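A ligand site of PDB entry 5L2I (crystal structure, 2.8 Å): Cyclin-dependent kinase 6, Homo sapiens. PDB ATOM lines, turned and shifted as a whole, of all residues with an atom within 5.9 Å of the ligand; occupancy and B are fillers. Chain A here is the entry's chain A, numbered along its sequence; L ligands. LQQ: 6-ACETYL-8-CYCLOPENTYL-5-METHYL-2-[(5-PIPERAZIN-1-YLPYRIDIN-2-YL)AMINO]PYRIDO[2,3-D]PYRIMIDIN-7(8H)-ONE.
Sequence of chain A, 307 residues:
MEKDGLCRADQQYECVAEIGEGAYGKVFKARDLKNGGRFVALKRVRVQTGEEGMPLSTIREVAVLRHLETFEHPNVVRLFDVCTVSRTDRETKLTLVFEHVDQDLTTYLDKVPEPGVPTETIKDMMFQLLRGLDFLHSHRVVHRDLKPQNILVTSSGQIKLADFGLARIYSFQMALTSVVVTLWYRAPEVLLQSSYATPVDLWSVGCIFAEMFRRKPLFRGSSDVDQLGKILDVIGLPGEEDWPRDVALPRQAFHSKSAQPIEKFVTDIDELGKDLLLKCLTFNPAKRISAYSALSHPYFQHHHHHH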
ATOM      1  N   GLU A  18      30.669 -20.053  -2.962  1.00  0.00           N
ATOM      2  CA  GLU A  18      30.570 -18.601  -2.769  1.00  0.00           C
ATOM      3  C   GLU A  18      29.989 -17.938  -4.041  1.00  0.00           C
ATOM      4  O   GLU A  18      30.627 -17.997  -5.097  1.00  0.00           O
ATOM      5  CB  GLU A  18      31.948 -18.031  -2.397  1.00  0.00           C
ATOM      6  CG  GLU A  18      31.904 -16.627  -1.802  1.00  0.00           C
ATOM      7  CD  GLU A  18      33.026 -15.739  -2.295  1.00  0.00           C
ATOM      8  OE1 GLU A  18      32.769 -14.913  -3.194  1.00  0.00           O
ATOM      9  OE2 GLU A  18      34.170 -15.893  -1.799  1.00  0.00           O
ATOM     10  N   ILE A  19      28.769 -17.348  -3.947  1.00  0.00           N
ATOM     11  CA  ILE A  19      28.056 -16.728  -5.079  1.00  0.00           C
ATOM     12  C   ILE A  19      28.729 -15.409  -5.495  1.00  0.00           C
ATOM     13  O   ILE A  19      29.152 -15.269  -6.650  1.00  0.00           O
ATOM     14  CB  ILE A  19      26.519 -16.560  -4.841  1.00  0.00           C
ATOM     15  CG1 ILE A  19      25.817 -17.929  -4.729  1.00  0.00           C
ATOM     16  CG2 ILE A  19      25.891 -15.747  -5.953  1.00  0.00           C
ATOM     17  CD1 ILE A  19      24.343 -17.882  -4.153  1.00  0.00           C
ATOM     18  N   GLY A  20      28.790 -14.452  -4.568  1.00  0.00           N
ATOM     19  CA  GLY A  20      29.385 -13.152  -4.798  1.00  0.00           C
ATOM     20  C   GLY A  20      30.007 -12.536  -3.561  1.00  0.00           C
ATOM     21  O   GLY A  20      29.606 -12.854  -2.436  1.00  0.00           O
ATOM     22  N   TYR A  24      28.960  -4.808   0.780  1.00  0.00           N
ATOM     23  CA  TYR A  24      27.707  -5.179   1.468  1.00  0.00           C
ATOM     24  C   TYR A  24      27.791  -6.558   2.204  1.00  0.00           C
ATOM     25  O   TYR A  24      26.918  -6.883   3.020  1.00  0.00           O
ATOM     26  CB  TYR A  24      26.534  -5.146   0.453  1.00  0.00           C
ATOM     27  CG  TYR A  24      26.732  -6.066  -0.735  1.00  0.00           C
ATOM     28  CD1 TYR A  24      26.179  -7.337  -0.762  1.00  0.00           C
ATOM     29  CD2 TYR A  24      27.514  -5.678  -1.823  1.00  0.00           C
ATOM     30  CE1 TYR A  24      26.391  -8.202  -1.834  1.00  0.00           C
ATOM     31  CE2 TYR A  24      27.745  -6.533  -2.897  1.00  0.00           C
ATOM     32  CZ  TYR A  24      27.183  -7.798  -2.898  1.00  0.00           C
ATOM     33  OH  TYR A  24      27.396  -8.643  -3.959  1.00  0.00           O
ATOM     34  N   VAL A  27      27.640 -13.404  -0.001  1.00  0.00           N
ATOM     35  CA  VAL A  27      26.456 -14.261  -0.143  1.00  0.00           C
ATOM     36  C   VAL A  27      26.920 -15.649  -0.609  1.00  0.00           C
ATOM     37  O   VAL A  27      27.818 -15.733  -1.448  1.00  0.00           O
ATOM     38  CB  VAL A  27      25.468 -13.590  -1.130  1.00  0.00           C
ATOM     39  CG1 VAL A  27      26.208 -13.046  -2.346  1.00  0.00           C
ATOM     40  CG2 VAL A  27      24.315 -14.522  -1.544  1.00  0.00           C
ATOM     41  N   ALA A  41      20.215 -19.428  -0.999  1.00  0.00           N
ATOM     42  CA  ALA A  41      21.203 -18.358  -0.921  1.00  0.00           C
ATOM     43  C   ALA A  41      21.172 -17.691   0.454  1.00  0.00           C
ATOM     44  O   ALA A  41      20.114 -17.206   0.866  1.00  0.00           O
ATOM     45  CB  ALA A  41      20.944 -17.331  -2.007  1.00  0.00           C
ATOM     46  N   LYS A  43      23.194 -14.929   3.319  1.00  0.00           N
ATOM     47  CA  LYS A  43      24.122 -13.819   3.551  1.00  0.00           C
ATOM     48  C   LYS A  43      23.965 -13.294   4.962  1.00  0.00           C
ATOM     49  O   LYS A  43      22.863 -12.978   5.409  1.00  0.00           O
ATOM     50  CB  LYS A  43      23.967 -12.696   2.504  1.00  0.00           C
ATOM     51  CG  LYS A  43      25.015 -11.574   2.623  1.00  0.00           C
ATOM     52  CD  LYS A  43      25.206 -10.751   1.345  1.00  0.00           C
ATOM     53  CE  LYS A  43      24.219  -9.614   1.189  1.00  0.00           C
ATOM     54  NZ  LYS A  43      24.638  -8.410   1.948  1.00  0.00           N
ATOM     55  N   VAL A  77      13.144 -12.344  -5.727  1.00  0.00           N
ATOM     56  CA  VAL A  77      13.597 -13.485  -4.918  1.00  0.00           C
ATOM     57  C   VAL A  77      12.785 -13.681  -3.619  1.00  0.00           C
ATOM     58  O   VAL A  77      12.520 -12.726  -2.890  1.00  0.00           O
ATOM     59  CB  VAL A  77      15.103 -13.487  -4.587  1.00  0.00           C
ATOM     60  CG1 VAL A  77      15.936 -13.991  -5.762  1.00  0.00           C
ATOM     61  CG2 VAL A  77      15.578 -12.127  -4.090  1.00  0.00           C
ATOM     62  N   ARG A  78      12.424 -14.931  -3.319  1.00  0.00           N
ATOM     63  CA  ARG A  78      11.700 -15.257  -2.092  1.00  0.00           C
ATOM     64  C   ARG A  78      12.688 -15.226  -0.955  1.00  0.00           C
ATOM     65  O   ARG A  78      13.858 -15.552  -1.138  1.00  0.00           O
ATOM     66  CB  ARG A  78      11.050 -16.664  -2.144  1.00  0.00           C
ATOM     67  CG  ARG A  78      10.092 -16.956  -3.333  1.00  0.00           C
ATOM     68  CD  ARG A  78       8.657 -16.480  -3.121  1.00  0.00           C
ATOM     69  NE  ARG A  78       8.544 -15.033  -3.214  1.00  0.00           N
ATOM     70  CZ  ARG A  78       8.437 -14.355  -4.359  1.00  0.00           C
ATOM     71  NH1 ARG A  78       8.414 -14.998  -5.519  1.00  0.00           N
ATOM     72  NH2 ARG A  78       8.353 -13.033  -4.344  1.00  0.00           N
ATOM     73  N   PHE A  98      17.375 -16.979   1.431  1.00  0.00           N
ATOM     74  CA  PHE A  98      16.484 -16.690   0.309  1.00  0.00           C
ATOM     75  C   PHE A  98      16.497 -17.849  -0.652  1.00  0.00           C
ATOM     76  O   PHE A  98      17.299 -18.779  -0.490  1.00  0.00           O
ATOM     77  CB  PHE A  98      17.032 -15.488  -0.500  1.00  0.00           C
ATOM     78  CG  PHE A  98      17.096 -14.130   0.134  1.00  0.00           C
ATOM     79  CD1 PHE A  98      16.125 -13.170  -0.133  1.00  0.00           C
ATOM     80  CD2 PHE A  98      18.171 -13.779   0.946  1.00  0.00           C
ATOM     81  CE1 PHE A  98      16.211 -11.899   0.431  1.00  0.00           C
ATOM     82  CE2 PHE A  98      18.261 -12.498   1.494  1.00  0.00           C
ATOM     83  CZ  PHE A  98      17.275 -11.569   1.229  1.00  0.00           C
ATOM     84  N   GLU A  99      15.683 -17.739  -1.736  1.00  0.00           N
ATOM     85  CA  GLU A  99      15.672 -18.729  -2.791  1.00  0.00           C
ATOM     86  C   GLU A  99      16.937 -18.618  -3.616  1.00  0.00           C
ATOM     87  O   GLU A  99      17.403 -17.508  -3.862  1.00  0.00           O
ATOM     88  CB  GLU A  99      14.419 -18.642  -3.671  1.00  0.00           C
ATOM     89  CG  GLU A  99      14.126 -17.321  -4.348  1.00  0.00           C
ATOM     90  CD  GLU A  99      13.204 -17.433  -5.556  1.00  0.00           C
ATOM     91  OE1 GLU A  99      12.285 -16.587  -5.694  1.00  0.00           O
ATOM     92  OE2 GLU A  99      13.416 -18.342  -6.396  1.00  0.00           O
ATOM     93  N   HIS A 100      17.524 -19.762  -3.989  1.00  0.00           N
ATOM     94  CA  HIS A 100      18.710 -19.805  -4.812  1.00  0.00           C
ATOM     95  C   HIS A 100      18.259 -19.899  -6.255  1.00  0.00           C
ATOM     96  O   HIS A 100      17.442 -20.751  -6.598  1.00  0.00           O
ATOM     97  CB  HIS A 100      19.580 -20.990  -4.423  1.00  0.00           C
ATOM     98  CG  HIS A 100      20.857 -21.115  -5.196  1.00  0.00           C
ATOM     99  ND1 HIS A 100      20.866 -21.313  -6.572  1.00  0.00           N
ATOM    100  CD2 HIS A 100      22.132 -21.134  -4.740  1.00  0.00           C
ATOM    101  CE1 HIS A 100      22.145 -21.409  -6.907  1.00  0.00           C
ATOM    102  NE2 HIS A 100      22.943 -21.297  -5.849  1.00  0.00           N
ATOM    103  N   VAL A 101      18.774 -18.997  -7.091  1.00  0.00           N
ATOM    104  CA  VAL A 101      18.501 -18.943  -8.534  1.00  0.00           C
ATOM    105  C   VAL A 101      19.752 -19.495  -9.220  1.00  0.00           C
ATOM    106  O   VAL A 101      20.841 -19.409  -8.676  1.00  0.00           O
ATOM    107  CB  VAL A 101      18.100 -17.539  -9.041  1.00  0.00           C
ATOM    108  CG1 VAL A 101      17.784 -17.552 -10.530  1.00  0.00           C
ATOM    109  CG2 VAL A 101      16.913 -16.970  -8.264  1.00  0.00           C
ATOM    110  N   ASP A 102      19.570 -20.096 -10.359  1.00  0.00           N
ATOM    111  CA  ASP A 102      20.606 -20.772 -11.119  1.00  0.00           C
ATOM    112  C   ASP A 102      21.772 -19.845 -11.512  1.00  0.00           C
ATOM    113  O   ASP A 102      22.916 -20.077 -11.120  1.00  0.00           O
ATOM    114  CB  ASP A 102      19.951 -21.499 -12.332  1.00  0.00           C
ATOM    115  CG  ASP A 102      18.755 -22.378 -11.917  1.00  0.00           C
ATOM    116  OD1 ASP A 102      17.693 -21.817 -11.520  1.00  0.00           O
ATOM    117  OD2 ASP A 102      18.905 -23.628 -11.925  1.00  0.00           O
ATOM    118  N   GLN A 103      21.463 -18.782 -12.236  1.00  0.00           N
ATOM    119  CA  GLN A 103      22.452 -17.831 -12.705  1.00  0.00           C
ATOM    120  C   GLN A 103      21.928 -16.372 -12.711  1.00  0.00           C
ATOM    121  O   GLN A 103      20.779 -16.128 -12.326  1.00  0.00           O
ATOM    122  CB  GLN A 103      22.964 -18.270 -14.109  1.00  0.00           C
ATOM    123  CG  GLN A 103      21.872 -18.691 -15.081  1.00  0.00           C
ATOM    124  CD  GLN A 103      22.253 -18.563 -16.530  1.00  0.00           C
ATOM    125  OE1 GLN A 103      21.581 -17.880 -17.303  1.00  0.00           O
ATOM    126  NE2 GLN A 103      23.309 -19.251 -16.943  1.00  0.00           N
ATOM    127  N   ASP A 104      22.789 -15.393 -13.104  1.00  0.00           N
ATOM    128  CA  ASP A 104      22.399 -13.983 -13.185  1.00  0.00           C
ATOM    129  C   ASP A 104      22.228 -13.577 -14.651  1.00  0.00           C
ATOM    130  O   ASP A 104      22.348 -14.427 -15.520  1.00  0.00           O
ATOM    131  CB  ASP A 104      23.366 -13.069 -12.416  1.00  0.00           C
ATOM    132  CG  ASP A 104      24.824 -13.096 -12.855  1.00  0.00           C
ATOM    133  OD1 ASP A 104      25.083 -13.437 -14.024  1.00  0.00           O
ATOM    134  OD2 ASP A 104      25.705 -12.748 -12.009  1.00  0.00           O
ATOM    135  N   THR A 107      26.078 -13.795 -16.583  1.00  0.00           N
ATOM    136  CA  THR A 107      26.471 -15.105 -17.098  1.00  0.00           C
ATOM    137  C   THR A 107      25.436 -15.655 -18.076  1.00  0.00           C
ATOM    138  O   THR A 107      25.775 -16.541 -18.858  1.00  0.00           O
ATOM    139  CB  THR A 107      26.880 -16.080 -16.014  1.00  0.00           C
ATOM    140  OG1 THR A 107      25.797 -16.964 -15.710  1.00  0.00           O
ATOM    141  CG2 THR A 107      27.436 -15.397 -14.796  1.00  0.00           C
ATOM    142  N   GLN A 149      24.365  -8.136 -12.726  1.00  0.00           N
ATOM    143  CA  GLN A 149      25.013  -9.000 -11.735  1.00  0.00           C
ATOM    144  C   GLN A 149      24.026  -9.496 -10.698  1.00  0.00           C
ATOM    145  O   GLN A 149      24.279 -10.550 -10.108  1.00  0.00           O
ATOM    146  CB  GLN A 149      26.215  -8.312 -11.080  1.00  0.00           C
ATOM    147  CG  GLN A 149      27.390  -8.086 -12.018  1.00  0.00           C
ATOM    148  CD  GLN A 149      27.358  -6.717 -12.668  1.00  0.00           C
ATOM    149  OE1 GLN A 149      26.461  -6.391 -13.465  1.00  0.00           O
ATOM    150  NE2 GLN A 149      28.344  -5.869 -12.343  1.00  0.00           N
ATOM    151  N   ASN A 150      22.889  -8.770 -10.499  1.00  0.00           N
ATOM    152  CA  ASN A 150      21.831  -9.090  -9.514  1.00  0.00           C
ATOM    153  C   ASN A 150      20.423  -9.175 -10.113  1.00  0.00           C
ATOM    154  O   ASN A 150      19.428  -9.093  -9.374  1.00  0.00           O
ATOM    155  CB  ASN A 150      21.854  -8.119  -8.316  1.00  0.00           C
ATOM    156  CG  ASN A 150      21.756  -6.650  -8.674  1.00  0.00           C
ATOM    157  OD1 ASN A 150      21.044  -6.236  -9.611  1.00  0.00           O
ATOM    158  ND2 ASN A 150      22.499  -5.839  -7.935  1.00  0.00           N
ATOM    159  N   ILE A 151      20.314  -9.315 -11.440  1.00  0.00           N
ATOM    160  CA  ILE A 151      19.049  -9.599 -12.118  1.00  0.00           C
ATOM    161  C   ILE A 151      19.250 -11.090 -12.362  1.00  0.00           C
ATOM    162  O   ILE A 151      20.112 -11.460 -13.162  1.00  0.00           O
ATOM    163  CB  ILE A 151      18.851  -8.811 -13.437  1.00  0.00           C
ATOM    164  CG1 ILE A 151      18.451  -7.379 -13.168  1.00  0.00           C
ATOM    165  CG2 ILE A 151      17.825  -9.487 -14.347  1.00  0.00           C
ATOM    166  CD1 ILE A 151      19.014  -6.456 -14.171  1.00  0.00           C
ATOM    167  N   LEU A 152      18.587 -11.948 -11.572  1.00  0.00           N
ATOM    168  CA  LEU A 152      18.767 -13.398 -11.680  1.00  0.00           C
ATOM    169  C   LEU A 152      17.819 -14.018 -12.707  1.00  0.00           C
ATOM    170  O   LEU A 152      16.835 -13.380 -13.082  1.00  0.00           O
ATOM    171  CB  LEU A 152      18.683 -14.078 -10.311  1.00  0.00           C
ATOM    172  CG  LEU A 152      19.537 -13.458  -9.195  1.00  0.00           C
ATOM    173  CD1 LEU A 152      19.180 -13.995  -7.863  1.00  0.00           C
ATOM    174  CD2 LEU A 152      21.008 -13.647  -9.446  1.00  0.00           C
ATOM    175  N   ALA A 162      16.912  -9.226  -7.272  1.00  0.00           N
ATOM    176  CA  ALA A 162      17.583  -9.594  -6.012  1.00  0.00           C
ATOM    177  C   ALA A 162      18.430  -8.421  -5.547  1.00  0.00           C
ATOM    178  O   ALA A 162      18.391  -7.368  -6.194  1.00  0.00           O
ATOM    179  CB  ALA A 162      18.451 -10.827  -6.213  1.00  0.00           C
ATOM    180  N   ASP A 163      19.178  -8.580  -4.422  1.00  0.00           N
ATOM    181  CA  ASP A 163      20.116  -7.623  -3.832  1.00  0.00           C
ATOM    182  C   ASP A 163      19.502  -6.255  -3.451  1.00  0.00           C
ATOM    183  O   ASP A 163      20.069  -5.221  -3.816  1.00  0.00           O
ATOM    184  CB  ASP A 163      21.345  -7.453  -4.758  1.00  0.00           C
ATOM    185  CG  ASP A 163      22.705  -7.421  -4.070  1.00  0.00           C
ATOM    186  OD1 ASP A 163      22.821  -8.005  -2.962  1.00  0.00           O
ATOM    187  OD2 ASP A 163      23.657  -6.872  -4.673  1.00  0.00           O
ATOM    188  N   PHE A 164      18.359  -6.257  -2.692  1.00  0.00           N
ATOM    189  CA  PHE A 164      17.662  -5.066  -2.148  1.00  0.00           C
ATOM    190  C   PHE A 164      17.240  -5.273  -0.646  1.00  0.00           C
ATOM    191  O   PHE A 164      17.123  -6.422  -0.175  1.00  0.00           O
ATOM    192  CB  PHE A 164      16.505  -4.571  -3.045  1.00  0.00           C
ATOM    193  CG  PHE A 164      15.413  -5.571  -3.324  1.00  0.00           C
ATOM    194  CD1 PHE A 164      14.316  -5.694  -2.476  1.00  0.00           C
ATOM    195  CD2 PHE A 164      15.478  -6.404  -4.438  1.00  0.00           C
ATOM    196  CE1 PHE A 164      13.328  -6.648  -2.711  1.00  0.00           C
ATOM    197  CE2 PHE A 164      14.482  -7.374  -4.671  1.00  0.00           C
ATOM    198  CZ  PHE A 164      13.410  -7.482  -3.810  1.00  0.00           C
HETATM  199  O01 LQQ L   1      19.158 -11.116  -2.715  1.00  0.00           O
HETATM  200  C02 LQQ L   1      20.264 -11.613  -2.495  1.00  0.00           C
HETATM  201  C01 LQQ L   1      21.023 -11.239  -1.257  1.00  0.00           C
HETATM  202  C03 LQQ L   1      20.847 -12.563  -3.446  1.00  0.00           C
HETATM  203  C04 LQQ L   1      20.265 -13.792  -3.651  1.00  0.00           C
HETATM  204  C05 LQQ L   1      19.128 -14.239  -2.788  1.00  0.00           C
HETATM  205  C06 LQQ L   1      20.792 -14.701  -4.659  1.00  0.00           C
HETATM  206  C07 LQQ L   1      20.205 -15.891  -5.112  1.00  0.00           C
HETATM  207  N01 LQQ L   1      20.657 -16.620  -6.133  1.00  0.00           N
HETATM  208  C08 LQQ L   1      21.799 -16.193  -6.692  1.00  0.00           C
HETATM  209  N02 LQQ L   1      22.483 -15.085  -6.375  1.00  0.00           N
HETATM  210  C09 LQQ L   1      21.949 -14.340  -5.381  1.00  0.00           C
HETATM  211  N03 LQQ L   1      22.539 -13.099  -5.144  1.00  0.00           N
HETATM  212  C10 LQQ L   1      23.681 -12.646  -5.991  1.00  0.00           C
HETATM  213  C11 LQQ L   1      23.305 -11.592  -7.036  1.00  0.00           C
HETATM  214  C12 LQQ L   1      24.535 -10.725  -7.114  1.00  0.00           C
HETATM  215  C13 LQQ L   1      25.092 -10.711  -5.734  1.00  0.00           C
HETATM  216  C14 LQQ L   1      24.884 -12.114  -5.216  1.00  0.00           C
HETATM  217  C15 LQQ L   1      22.016 -12.171  -4.195  1.00  0.00           C
HETATM  218  O02 LQQ L   1      22.535 -11.064  -4.036  1.00  0.00           O
HETATM  219  N04 LQQ L   1      22.273 -17.036  -7.659  1.00  0.00           N
HETATM  220  C16 LQQ L   1      23.444 -17.014  -8.388  1.00  0.00           C
HETATM  221  N05 LQQ L   1      24.298 -17.976  -8.025  1.00  0.00           N
HETATM  222  C17 LQQ L   1      25.478 -18.038  -8.650  1.00  0.00           C
HETATM  223  C18 LQQ L   1      25.876 -17.152  -9.645  1.00  0.00           C
HETATM  224  C19 LQQ L   1      24.966 -16.171 -10.019  1.00  0.00           C
HETATM  225  C20 LQQ L   1      23.736 -16.081  -9.398  1.00  0.00           C
HETATM  226  N06 LQQ L   1      27.167 -17.213 -10.179  1.00  0.00           N
HETATM  227  C21 LQQ L   1      27.351 -16.863 -11.593  1.00  0.00           C
HETATM  228  C22 LQQ L   1      28.701 -17.343 -12.079  1.00  0.00           C
HETATM  229  N07 LQQ L   1      29.772 -16.775 -11.224  1.00  0.00           N
HETATM  230  C23 LQQ L   1      29.583 -17.158  -9.796  1.00  0.00           C
HETATM  231  C24 LQQ L   1      28.226 -16.690  -9.318  1.00  0.00           C
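O of Ile 19 touches C24 of the ligand, 3.2 Å away.
Tyr 24 touches the ligand (OH to C13, 3.6 Å).
Val 27 touches the ligand.
CB of Ala 41 touches C07 of the ligand (3.5 Å).
Val 77 touches the ligand.
Phe 98 touches the ligand (CB to C05, 3.3 Å).
Glu 99 touches the ligand (O to C07, 3.5 Å).
His 100 touches the ligand (CA to N01, 3.96 Å).
Asp 102 touches the ligand (O to N05, 3.99 Å).
C of Gln 103 touches C20 of the ligand, at 3.8 Å.
Asp 104 touches the ligand (N to C19, 3.9 Å).
CG2 of Thr 107 touches C21 of the ligand (3.5 Å).
O of Gln 149 touches C12 of the ligand (3.0 Å).
Asn 150 touches the ligand (CA to C11, 3.8 Å).
Leu 152 touches the ligand.
Ala 162 touches the ligand.
Hydrophobic or aromatic side chains that line the ligand: Ile 19, Val 27, Ala 41, Val 77, Phe 98, Val 101, Leu 152 and Ala 162.
18 residues have an atom within 4 Å of the ligand: Ile 19, Tyr 24, Val 27, Ala 41, Val 77, Phe 98, Glu 99, His 100, Val 101, Asp 102, Gln 103, Asp 104, Thr 107, Gln 149, Asn 150, Leu 152, Ala 162 and Asp 163.
O of Gly 20 lies within hydrogen-bond range of N of Val 27 (3.2 Å).
OE1 of Glu 99 is in hydrogen-bond range of N of Arg 78 (2.9 Å).
The backbone carbonyl oxygen (O) of Tyr 24 is in hydrogen-bond range of the side-chain amino group (NZ) of Lys 43, at 2.9 Å.
The backbone NH (N) of Ile 19 sits at hydrogen-bond distance from the backbone carbonyl oxygen (O) of Val 27 (3.1 Å).
The backbone carbonyl oxygen (O) of Ala 41 is in hydrogen-bond range of the backbone NH (N) of Phe 98 (2.8 Å).
The backbone carbonyl oxygen (O) of Asn 150 sits at hydrogen-bond distance from the backbone NH (N) of Ala 162, at 3.3 Å.
The backbone NH (N) of Thr 107 is in hydrogen-bond range of the side-chain carboxylate (OD1) of Asp 104.
N of Val 101 lies within hydrogen-bond range of N01 of the ligand (3.2 Å).
N04 of the ligand sits close to O of Val 101 (3.0 Å).
The backbone NH (N) of Asp 163 lies within hydrogen-bond range of an oxygen (O01) of the ligand, 3.1 Å away.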
